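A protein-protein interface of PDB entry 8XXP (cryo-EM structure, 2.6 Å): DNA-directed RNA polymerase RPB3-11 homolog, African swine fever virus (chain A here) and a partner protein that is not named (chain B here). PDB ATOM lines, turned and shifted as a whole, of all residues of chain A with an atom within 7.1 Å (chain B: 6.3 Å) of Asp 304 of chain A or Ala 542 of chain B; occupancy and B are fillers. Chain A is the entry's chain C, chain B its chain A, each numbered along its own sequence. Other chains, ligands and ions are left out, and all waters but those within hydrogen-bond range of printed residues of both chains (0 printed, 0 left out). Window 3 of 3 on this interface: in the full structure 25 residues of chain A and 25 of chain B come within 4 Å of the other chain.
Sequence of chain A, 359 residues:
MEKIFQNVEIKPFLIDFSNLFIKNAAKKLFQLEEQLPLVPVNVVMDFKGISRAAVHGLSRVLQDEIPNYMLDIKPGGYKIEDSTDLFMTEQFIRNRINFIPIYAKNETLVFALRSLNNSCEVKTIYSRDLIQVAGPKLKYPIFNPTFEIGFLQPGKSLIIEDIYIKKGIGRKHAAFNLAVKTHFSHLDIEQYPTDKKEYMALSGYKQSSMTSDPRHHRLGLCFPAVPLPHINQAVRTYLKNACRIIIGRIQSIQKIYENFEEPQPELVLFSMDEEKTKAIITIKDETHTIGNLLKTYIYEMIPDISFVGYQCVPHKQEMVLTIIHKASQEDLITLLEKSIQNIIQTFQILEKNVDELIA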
ATOM      1  N   LYS A 276      -9.886 -16.284  18.796  1.00  0.00           N
ATOM      2  CA  LYS A 276      -8.960 -17.340  18.422  1.00  0.00           C
ATOM      3  C   LYS A 276      -7.873 -16.749  17.543  1.00  0.00           C
ATOM      4  O   LYS A 276      -8.169 -16.029  16.585  1.00  0.00           O
ATOM      5  CB  LYS A 276      -9.678 -18.468  17.680  1.00  0.00           C
ATOM      6  CG  LYS A 276     -10.489 -19.391  18.564  1.00  0.00           C
ATOM      7  CD  LYS A 276     -11.005 -20.611  17.820  1.00  0.00           C
ATOM      8  CE  LYS A 276     -11.559 -20.237  16.456  1.00  0.00           C
ATOM      9  NZ  LYS A 276     -12.395 -21.330  15.874  1.00  0.00           N
ATOM     10  N   ILE A 298       3.381 -28.072  23.528  1.00  0.00           N
ATOM     11  CA  ILE A 298       2.321 -27.077  23.440  1.00  0.00           C
ATOM     12  C   ILE A 298       1.036 -27.639  24.019  1.00  0.00           C
ATOM     13  O   ILE A 298       0.330 -26.967  24.779  1.00  0.00           O
ATOM     14  CB  ILE A 298       2.137 -26.626  21.982  1.00  0.00           C
ATOM     15  CG1 ILE A 298       3.314 -25.761  21.544  1.00  0.00           C
ATOM     16  CG2 ILE A 298       0.840 -25.869  21.821  1.00  0.00           C
ATOM     17  CD1 ILE A 298       3.447 -25.615  20.054  1.00  0.00           C
ATOM     18  N   TYR A 299       0.720 -28.887  23.681  1.00  0.00           N
ATOM     19  CA  TYR A 299      -0.472 -29.532  24.211  1.00  0.00           C
ATOM     20  C   TYR A 299      -0.395 -29.697  25.721  1.00  0.00           C
ATOM     21  O   TYR A 299      -1.378 -29.457  26.430  1.00  0.00           O
ATOM     22  CB  TYR A 299      -0.639 -30.882  23.530  1.00  0.00           C
ATOM     23  CG  TYR A 299      -1.868 -31.641  23.919  1.00  0.00           C
ATOM     24  CD1 TYR A 299      -3.126 -31.115  23.698  1.00  0.00           C
ATOM     25  CD2 TYR A 299      -1.772 -32.899  24.477  1.00  0.00           C
ATOM     26  CE1 TYR A 299      -4.244 -31.811  24.036  1.00  0.00           C
ATOM     27  CE2 TYR A 299      -2.886 -33.598  24.819  1.00  0.00           C
ATOM     28  CZ  TYR A 299      -4.117 -33.052  24.593  1.00  0.00           C
ATOM     29  OH  TYR A 299      -5.230 -33.759  24.926  1.00  0.00           O
ATOM     30  N   MET A 301       1.184 -27.845  27.695  1.00  0.00           N
ATOM     31  CA  MET A 301       1.171 -26.532  28.321  1.00  0.00           C
ATOM     32  C   MET A 301      -0.164 -25.826  28.136  1.00  0.00           C
ATOM     33  O   MET A 301      -0.533 -24.977  28.955  1.00  0.00           O
ATOM     34  CB  MET A 301       2.318 -25.703  27.751  1.00  0.00           C
ATOM     35  CG  MET A 301       2.404 -24.290  28.235  1.00  0.00           C
ATOM     36  SD  MET A 301       3.128 -24.372  29.868  1.00  0.00           S
ATOM     37  CE  MET A 301       4.847 -24.366  29.416  1.00  0.00           C
ATOM     38  N   ILE A 302      -0.901 -26.168  27.086  1.00  0.00           N
ATOM     39  CA  ILE A 302      -2.228 -25.618  26.834  1.00  0.00           C
ATOM     40  C   ILE A 302      -3.199 -26.782  26.683  1.00  0.00           C
ATOM     41  O   ILE A 302      -3.579 -27.120  25.557  1.00  0.00           O
ATOM     42  CB  ILE A 302      -2.244 -24.730  25.583  1.00  0.00           C
ATOM     43  CG1 ILE A 302      -1.010 -23.829  25.537  1.00  0.00           C
ATOM     44  CG2 ILE A 302      -3.499 -23.900  25.547  1.00  0.00           C
ATOM     45  CD1 ILE A 302      -0.899 -23.008  24.279  1.00  0.00           C
ATOM     46  N   PRO A 303      -3.611 -27.430  27.772  1.00  0.00           N
ATOM     47  CA  PRO A 303      -4.515 -28.582  27.633  1.00  0.00           C
ATOM     48  C   PRO A 303      -5.841 -28.240  26.980  1.00  0.00           C
ATOM     49  O   PRO A 303      -6.423 -29.091  26.300  1.00  0.00           O
ATOM     50  CB  PRO A 303      -4.697 -29.061  29.079  1.00  0.00           C
ATOM     51  CG  PRO A 303      -4.324 -27.898  29.923  1.00  0.00           C
ATOM     52  CD  PRO A 303      -3.285 -27.143  29.177  1.00  0.00           C
ATOM     53  N   ASP A 304      -6.336 -27.015  27.160  1.00  0.00           N
ATOM     54  CA  ASP A 304      -7.586 -26.569  26.560  1.00  0.00           C
ATOM     55  C   ASP A 304      -7.385 -25.914  25.202  1.00  0.00           C
ATOM     56  O   ASP A 304      -8.168 -25.040  24.820  1.00  0.00           O
ATOM     57  CB  ASP A 304      -8.305 -25.607  27.506  1.00  0.00           C
ATOM     58  CG  ASP A 304      -7.502 -24.352  27.784  1.00  0.00           C
ATOM     59  OD1 ASP A 304      -6.297 -24.466  28.093  1.00  0.00           O
ATOM     60  OD2 ASP A 304      -8.074 -23.247  27.692  1.00  0.00           O
ATOM     61  N   ILE A 305      -6.343 -26.302  24.470  1.00  0.00           N
ATOM     62  CA  ILE A 305      -6.049 -25.693  23.182  1.00  0.00           C
ATOM     63  C   ILE A 305      -7.147 -26.032  22.184  1.00  0.00           C
ATOM     64  O   ILE A 305      -7.716 -27.129  22.203  1.00  0.00           O
ATOM     65  CB  ILE A 305      -4.669 -26.158  22.681  1.00  0.00           C
ATOM     66  CG1 ILE A 305      -4.235 -25.354  21.459  1.00  0.00           C
ATOM     67  CG2 ILE A 305      -4.663 -27.646  22.390  1.00  0.00           C
ATOM     68  CD1 ILE A 305      -2.756 -25.333  21.252  1.00  0.00           C
ATOM     69  N   SER A 306      -7.470 -25.074  21.319  1.00  0.00           N
ATOM     70  CA  SER A 306      -8.453 -25.334  20.275  1.00  0.00           C
ATOM     71  C   SER A 306      -7.928 -26.354  19.276  1.00  0.00           C
ATOM     72  O   SER A 306      -8.626 -27.311  18.928  1.00  0.00           O
ATOM     73  CB  SER A 306      -8.835 -24.030  19.578  1.00  0.00           C
ATOM     74  OG  SER A 306      -9.755 -24.265  18.533  1.00  0.00           O
ATOM     75  N   PHE A 307      -6.693 -26.176  18.816  1.00  0.00           N
ATOM     76  CA  PHE A 307      -6.067 -27.140  17.925  1.00  0.00           C
ATOM     77  C   PHE A 307      -4.560 -26.951  17.962  1.00  0.00           C
ATOM     78  O   PHE A 307      -4.075 -25.820  17.956  1.00  0.00           O
ATOM     79  CB  PHE A 307      -6.571 -26.997  16.486  1.00  0.00           C
ATOM     80  CG  PHE A 307      -5.918 -27.942  15.523  1.00  0.00           C
ATOM     81  CD1 PHE A 307      -6.320 -29.259  15.448  1.00  0.00           C
ATOM     82  CD2 PHE A 307      -4.890 -27.517  14.704  1.00  0.00           C
ATOM     83  CE1 PHE A 307      -5.716 -30.129  14.574  1.00  0.00           C
ATOM     84  CE2 PHE A 307      -4.287 -28.387  13.828  1.00  0.00           C
ATOM     85  CZ  PHE A 307      -4.701 -29.693  13.765  1.00  0.00           C
ATOM     86  N   ILE A 324      -3.904 -23.245  17.106  1.00  0.00           N
ATOM     87  CA  ILE A 324      -5.100 -22.426  17.232  1.00  0.00           C
ATOM     88  C   ILE A 324      -5.517 -22.442  18.690  1.00  0.00           C
ATOM     89  O   ILE A 324      -5.709 -23.512  19.273  1.00  0.00           O
ATOM     90  CB  ILE A 324      -6.238 -22.924  16.326  1.00  0.00           C
ATOM     91  CG1 ILE A 324      -5.755 -23.016  14.883  1.00  0.00           C
ATOM     92  CG2 ILE A 324      -7.433 -22.007  16.432  1.00  0.00           C
ATOM     93  CD1 ILE A 324      -6.813 -23.456  13.927  1.00  0.00           C
ATOM     94  N   HIS A 325      -5.642 -21.259  19.281  1.00  0.00           N
ATOM     95  CA  HIS A 325      -5.930 -21.163  20.698  1.00  0.00           C
ATOM     96  C   HIS A 325      -6.819 -19.958  20.948  1.00  0.00           C
ATOM     97  O   HIS A 325      -6.774 -18.971  20.213  1.00  0.00           O
ATOM     98  CB  HIS A 325      -4.639 -21.068  21.518  1.00  0.00           C
ATOM     99  CG  HIS A 325      -4.861 -21.046  22.997  1.00  0.00           C
ATOM    100  ND1 HIS A 325      -5.910 -21.700  23.602  1.00  0.00           N
ATOM    101  CD2 HIS A 325      -4.165 -20.449  23.991  1.00  0.00           C
ATOM    102  CE1 HIS A 325      -5.854 -21.503  24.905  1.00  0.00           C
ATOM    103  NE2 HIS A 325      -4.804 -20.748  25.169  1.00  0.00           N
ATOM    104  N   LYS A 326      -7.635 -20.060  21.995  1.00  0.00           N
ATOM    105  CA  LYS A 326      -8.547 -18.996  22.406  1.00  0.00           C
ATOM    106  C   LYS A 326      -7.783 -18.001  23.282  1.00  0.00           C
ATOM    107  O   LYS A 326      -7.985 -17.888  24.492  1.00  0.00           O
ATOM    108  CB  LYS A 326      -9.744 -19.589  23.134  1.00  0.00           C
ATOM    109  CG  LYS A 326     -10.986 -18.730  23.105  1.00  0.00           C
ATOM    110  CD  LYS A 326     -11.713 -18.900  21.791  1.00  0.00           C
ATOM    111  CE  LYS A 326     -12.224 -20.317  21.595  1.00  0.00           C
ATOM    112  NZ  LYS A 326     -13.443 -20.594  22.396  1.00  0.00           N
ATOM    113  N   LYS B 524      -7.914 -36.536  23.148  1.00  0.00           N
ATOM    114  CA  LYS B 524      -7.952 -35.276  22.412  1.00  0.00           C
ATOM    115  C   LYS B 524      -6.726 -35.106  21.529  1.00  0.00           C
ATOM    116  O   LYS B 524      -6.820 -34.563  20.423  1.00  0.00           O
ATOM    117  CB  LYS B 524      -8.072 -34.109  23.387  1.00  0.00           C
ATOM    118  CG  LYS B 524      -7.901 -32.757  22.739  1.00  0.00           C
ATOM    119  CD  LYS B 524      -8.008 -31.648  23.741  1.00  0.00           C
ATOM    120  CE  LYS B 524      -7.769 -30.312  23.086  1.00  0.00           C
ATOM    121  NZ  LYS B 524      -8.091 -29.200  24.000  1.00  0.00           N
ATOM    122  N   CYS B 540     -12.566 -27.375  16.196  1.00  0.00           N
ATOM    123  CA  CYS B 540     -12.232 -26.857  17.512  1.00  0.00           C
ATOM    124  C   CYS B 540     -12.323 -27.992  18.523  1.00  0.00           C
ATOM    125  O   CYS B 540     -13.352 -28.665  18.616  1.00  0.00           O
ATOM    126  CB  CYS B 540     -13.163 -25.709  17.897  1.00  0.00           C
ATOM    127  SG  CYS B 540     -12.598 -24.690  19.270  1.00  0.00           S
ATOM    128  N   PHE B 541     -11.240 -28.211  19.262  1.00  0.00           N
ATOM    129  CA  PHE B 541     -11.217 -29.179  20.346  1.00  0.00           C
ATOM    130  C   PHE B 541     -11.133 -28.507  21.706  1.00  0.00           C
ATOM    131  O   PHE B 541     -10.880 -29.186  22.703  1.00  0.00           O
ATOM    132  CB  PHE B 541     -10.050 -30.148  20.173  1.00  0.00           C
ATOM    133  CG  PHE B 541     -10.155 -31.016  18.960  1.00  0.00           C
ATOM    134  CD1 PHE B 541      -9.780 -30.542  17.718  1.00  0.00           C
ATOM    135  CD2 PHE B 541     -10.616 -32.311  19.061  1.00  0.00           C
ATOM    136  CE1 PHE B 541      -9.869 -31.340  16.607  1.00  0.00           C
ATOM    137  CE2 PHE B 541     -10.710 -33.105  17.950  1.00  0.00           C
ATOM    138  CZ  PHE B 541     -10.333 -32.621  16.723  1.00  0.00           C
ATOM    139  N   ALA B 542     -11.343 -27.190  21.767  1.00  0.00           N
ATOM    140  CA  ALA B 542     -11.169 -26.442  23.005  1.00  0.00           C
ATOM    141  C   ALA B 542     -12.148 -26.859  24.087  1.00  0.00           C
ATOM    142  O   ALA B 542     -11.885 -26.616  25.267  1.00  0.00           O
ATOM    143  CB  ALA B 542     -11.310 -24.946  22.739  1.00  0.00           C
ATOM    144  N   ASN B 543     -13.264 -27.475  23.721  1.00  0.00           N
ATOM    145  CA  ASN B 543     -14.231 -27.963  24.691  1.00  0.00           C
ATOM    146  C   ASN B 543     -13.883 -29.343  25.223  1.00  0.00           C
ATOM    147  O   ASN B 543     -14.625 -29.876  26.050  1.00  0.00           O
ATOM    148  CB  ASN B 543     -15.630 -27.984  24.073  1.00  0.00           C
ATOM    149  CG  ASN B 543     -15.619 -28.430  22.624  1.00  0.00           C
ATOM    150  OD1 ASN B 543     -14.760 -28.025  21.842  1.00  0.00           O
ATOM    151  ND2 ASN B 543     -16.582 -29.265  22.258  1.00  0.00           N
ATOM    152  N   TYR B 544     -12.780 -29.934  24.775  1.00  0.00           N
ATOM    153  CA  TYR B 544     -12.370 -31.263  25.198  1.00  0.00           C
ATOM    154  C   TYR B 544     -11.165 -31.161  26.120  1.00  0.00           C
ATOM    155  O   TYR B 544     -10.214 -30.431  25.828  1.00  0.00           O
ATOM    156  CB  TYR B 544     -12.038 -32.143  23.994  1.00  0.00           C
ATOM    157  CG  TYR B 544     -13.231 -32.442  23.129  1.00  0.00           C
ATOM    158  CD1 TYR B 544     -14.151 -33.408  23.495  1.00  0.00           C
ATOM    159  CD2 TYR B 544     -13.443 -31.751  21.950  1.00  0.00           C
ATOM    160  CE1 TYR B 544     -15.242 -33.677  22.709  1.00  0.00           C
ATOM    161  CE2 TYR B 544     -14.526 -32.015  21.158  1.00  0.00           C
ATOM    162  CZ  TYR B 544     -15.426 -32.976  21.540  1.00  0.00           C
ATOM    163  OH  TYR B 544     -16.514 -33.238  20.747  1.00  0.00           O
ATOM    164  N   SER B 545     -11.224 -31.876  27.237  1.00  0.00           N
ATOM    165  CA  SER B 545     -10.077 -32.007  28.112  1.00  0.00           C
ATOM    166  C   SER B 545      -9.078 -32.984  27.501  1.00  0.00           C
ATOM    167  O   SER B 545      -9.431 -33.776  26.627  1.00  0.00           O
ATOM    168  CB  SER B 545     -10.511 -32.498  29.489  1.00  0.00           C
ATOM    169  OG  SER B 545     -11.770 -31.961  29.850  1.00  0.00           O
ATOM    170  N   PRO B 546      -7.819 -32.939  27.935  1.00  0.00           N
ATOM    171  CA  PRO B 546      -6.850 -33.916  27.427  1.00  0.00           C
ATOM    172  C   PRO B 546      -7.248 -35.362  27.658  1.00  0.00           C
ATOM    173  O   PRO B 546      -6.930 -36.215  26.824  1.00  0.00           O
ATOM    174  CB  PRO B 546      -5.556 -33.551  28.170  1.00  0.00           C
ATOM    175  CG  PRO B 546      -5.953 -32.582  29.227  1.00  0.00           C
ATOM    176  CD  PRO B 546      -7.157 -31.882  28.709  1.00  0.00           C
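The side-chain amino group (NZ) of Lys 524 of chain B is in hydrogen-bond range of the backbone carbonyl oxygen (O) of Phe 541 of chain B, at 3.1 Å.
NZ of Lys 524 of chain B sits at hydrogen-bond distance from O of Tyr 544 of chain B, at 3.1 Å.
The side-chain sulfur of Cys 540 of chain B lies close to the backbone NH of Ala 542 of chain B (3.7 Å).
N of Ser 306 of chain A is in hydrogen-bond range of O of Ile 324 of chain A.
Printed residues of chain B that touch a printed residue of chain A: Lys 524, Cys 540, Phe 541, Ala 542 and Pro 546.
Hydrophobic or aromatic side chains of chain B within 4 Å of the printed part of chain A: Phe 541, Ala 542 and Pro 546.
Along chain B the printed residues that touch a printed residue of chain A span positions 524 to 546.
Along chain A the printed residues that touch a printed residue of chain B span positions 299 to 306.
Among the printed residues, no Asp or Glu carboxylate lies within 4 Å of a Lys or Arg side-chain nitrogen of the other chain.
The side-chain amino group (NZ) of Lys 524 of chain B is in hydrogen-bond range of the backbone carbonyl oxygen (O) of Pro 303 of chain A, at 2.8 Å.
O of Ile 305 of chain A lies within hydrogen-bond range of NZ of Lys 524 of chain B.
The side-chain sulfur (SG) of Cys 540 of chain B lies within hydrogen-bond range of the side-chain hydroxyl (OG) of Ser 306 of chain A, 3.0 Å away.
O of Ser 306 of chain A lies within hydrogen-bond range of N of Phe 541 of chain B.
Of the printed residues of chain B, Tyr 299 of chain A touches Lys 524 and Pro 546.
Ile 302 of chain A touches none of the printed residues of chain B.
Of the printed residues of chain B, Pro 303 of chain A touches Lys 524 and Pro 546.
Asp 304 of chain A touches two residues of chain B.
Printed residues of chain B within 4 Å of Ile 305 of chain A: Lys 524 (2.8 Å), Phe 541 (3.7 Å) and Ala 542 (3.6 Å).
Of the printed residues of chain A, Phe 541 of chain B touches Ile 305 and Ser 306.
Ala 542 of chain B touches just these residues of chain A: Asp 304, Ile 305 and Ser 306.
The nearest residue of chain B that does not touch Asp 304 of chain A is Tyr 544 of chain B (4.7 Å).
The nearest residue of chain A that does not touch Ala 542 of chain B is Lys 326 of chain A (4.9 Å).
The nearest printed residue of chain A that does not touch Lys 524 of chain B is Ser 306 of chain A (5.0 Å).
Tyr 299 of chain A touches Lys 524 of chain B (OH to CB, 3.3 Å).
Tyr 299 of chain A touches Pro 546 of chain B.
Pro 546 of chain B touches Pro 303 of chain A.
Lys 524 of chain B touches Asp 304 of chain A.
Asp 304 of chain A touches Ala 542 of chain B.
Ile 305 of chain A touches Phe 541 of chain B (O to C, 3.7 Å).
CA of Ala 542 of chain B touches O of Ile 305 of chain A (3.6 Å).
Ser 306 of chain A touches Ala 542 of chain B.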
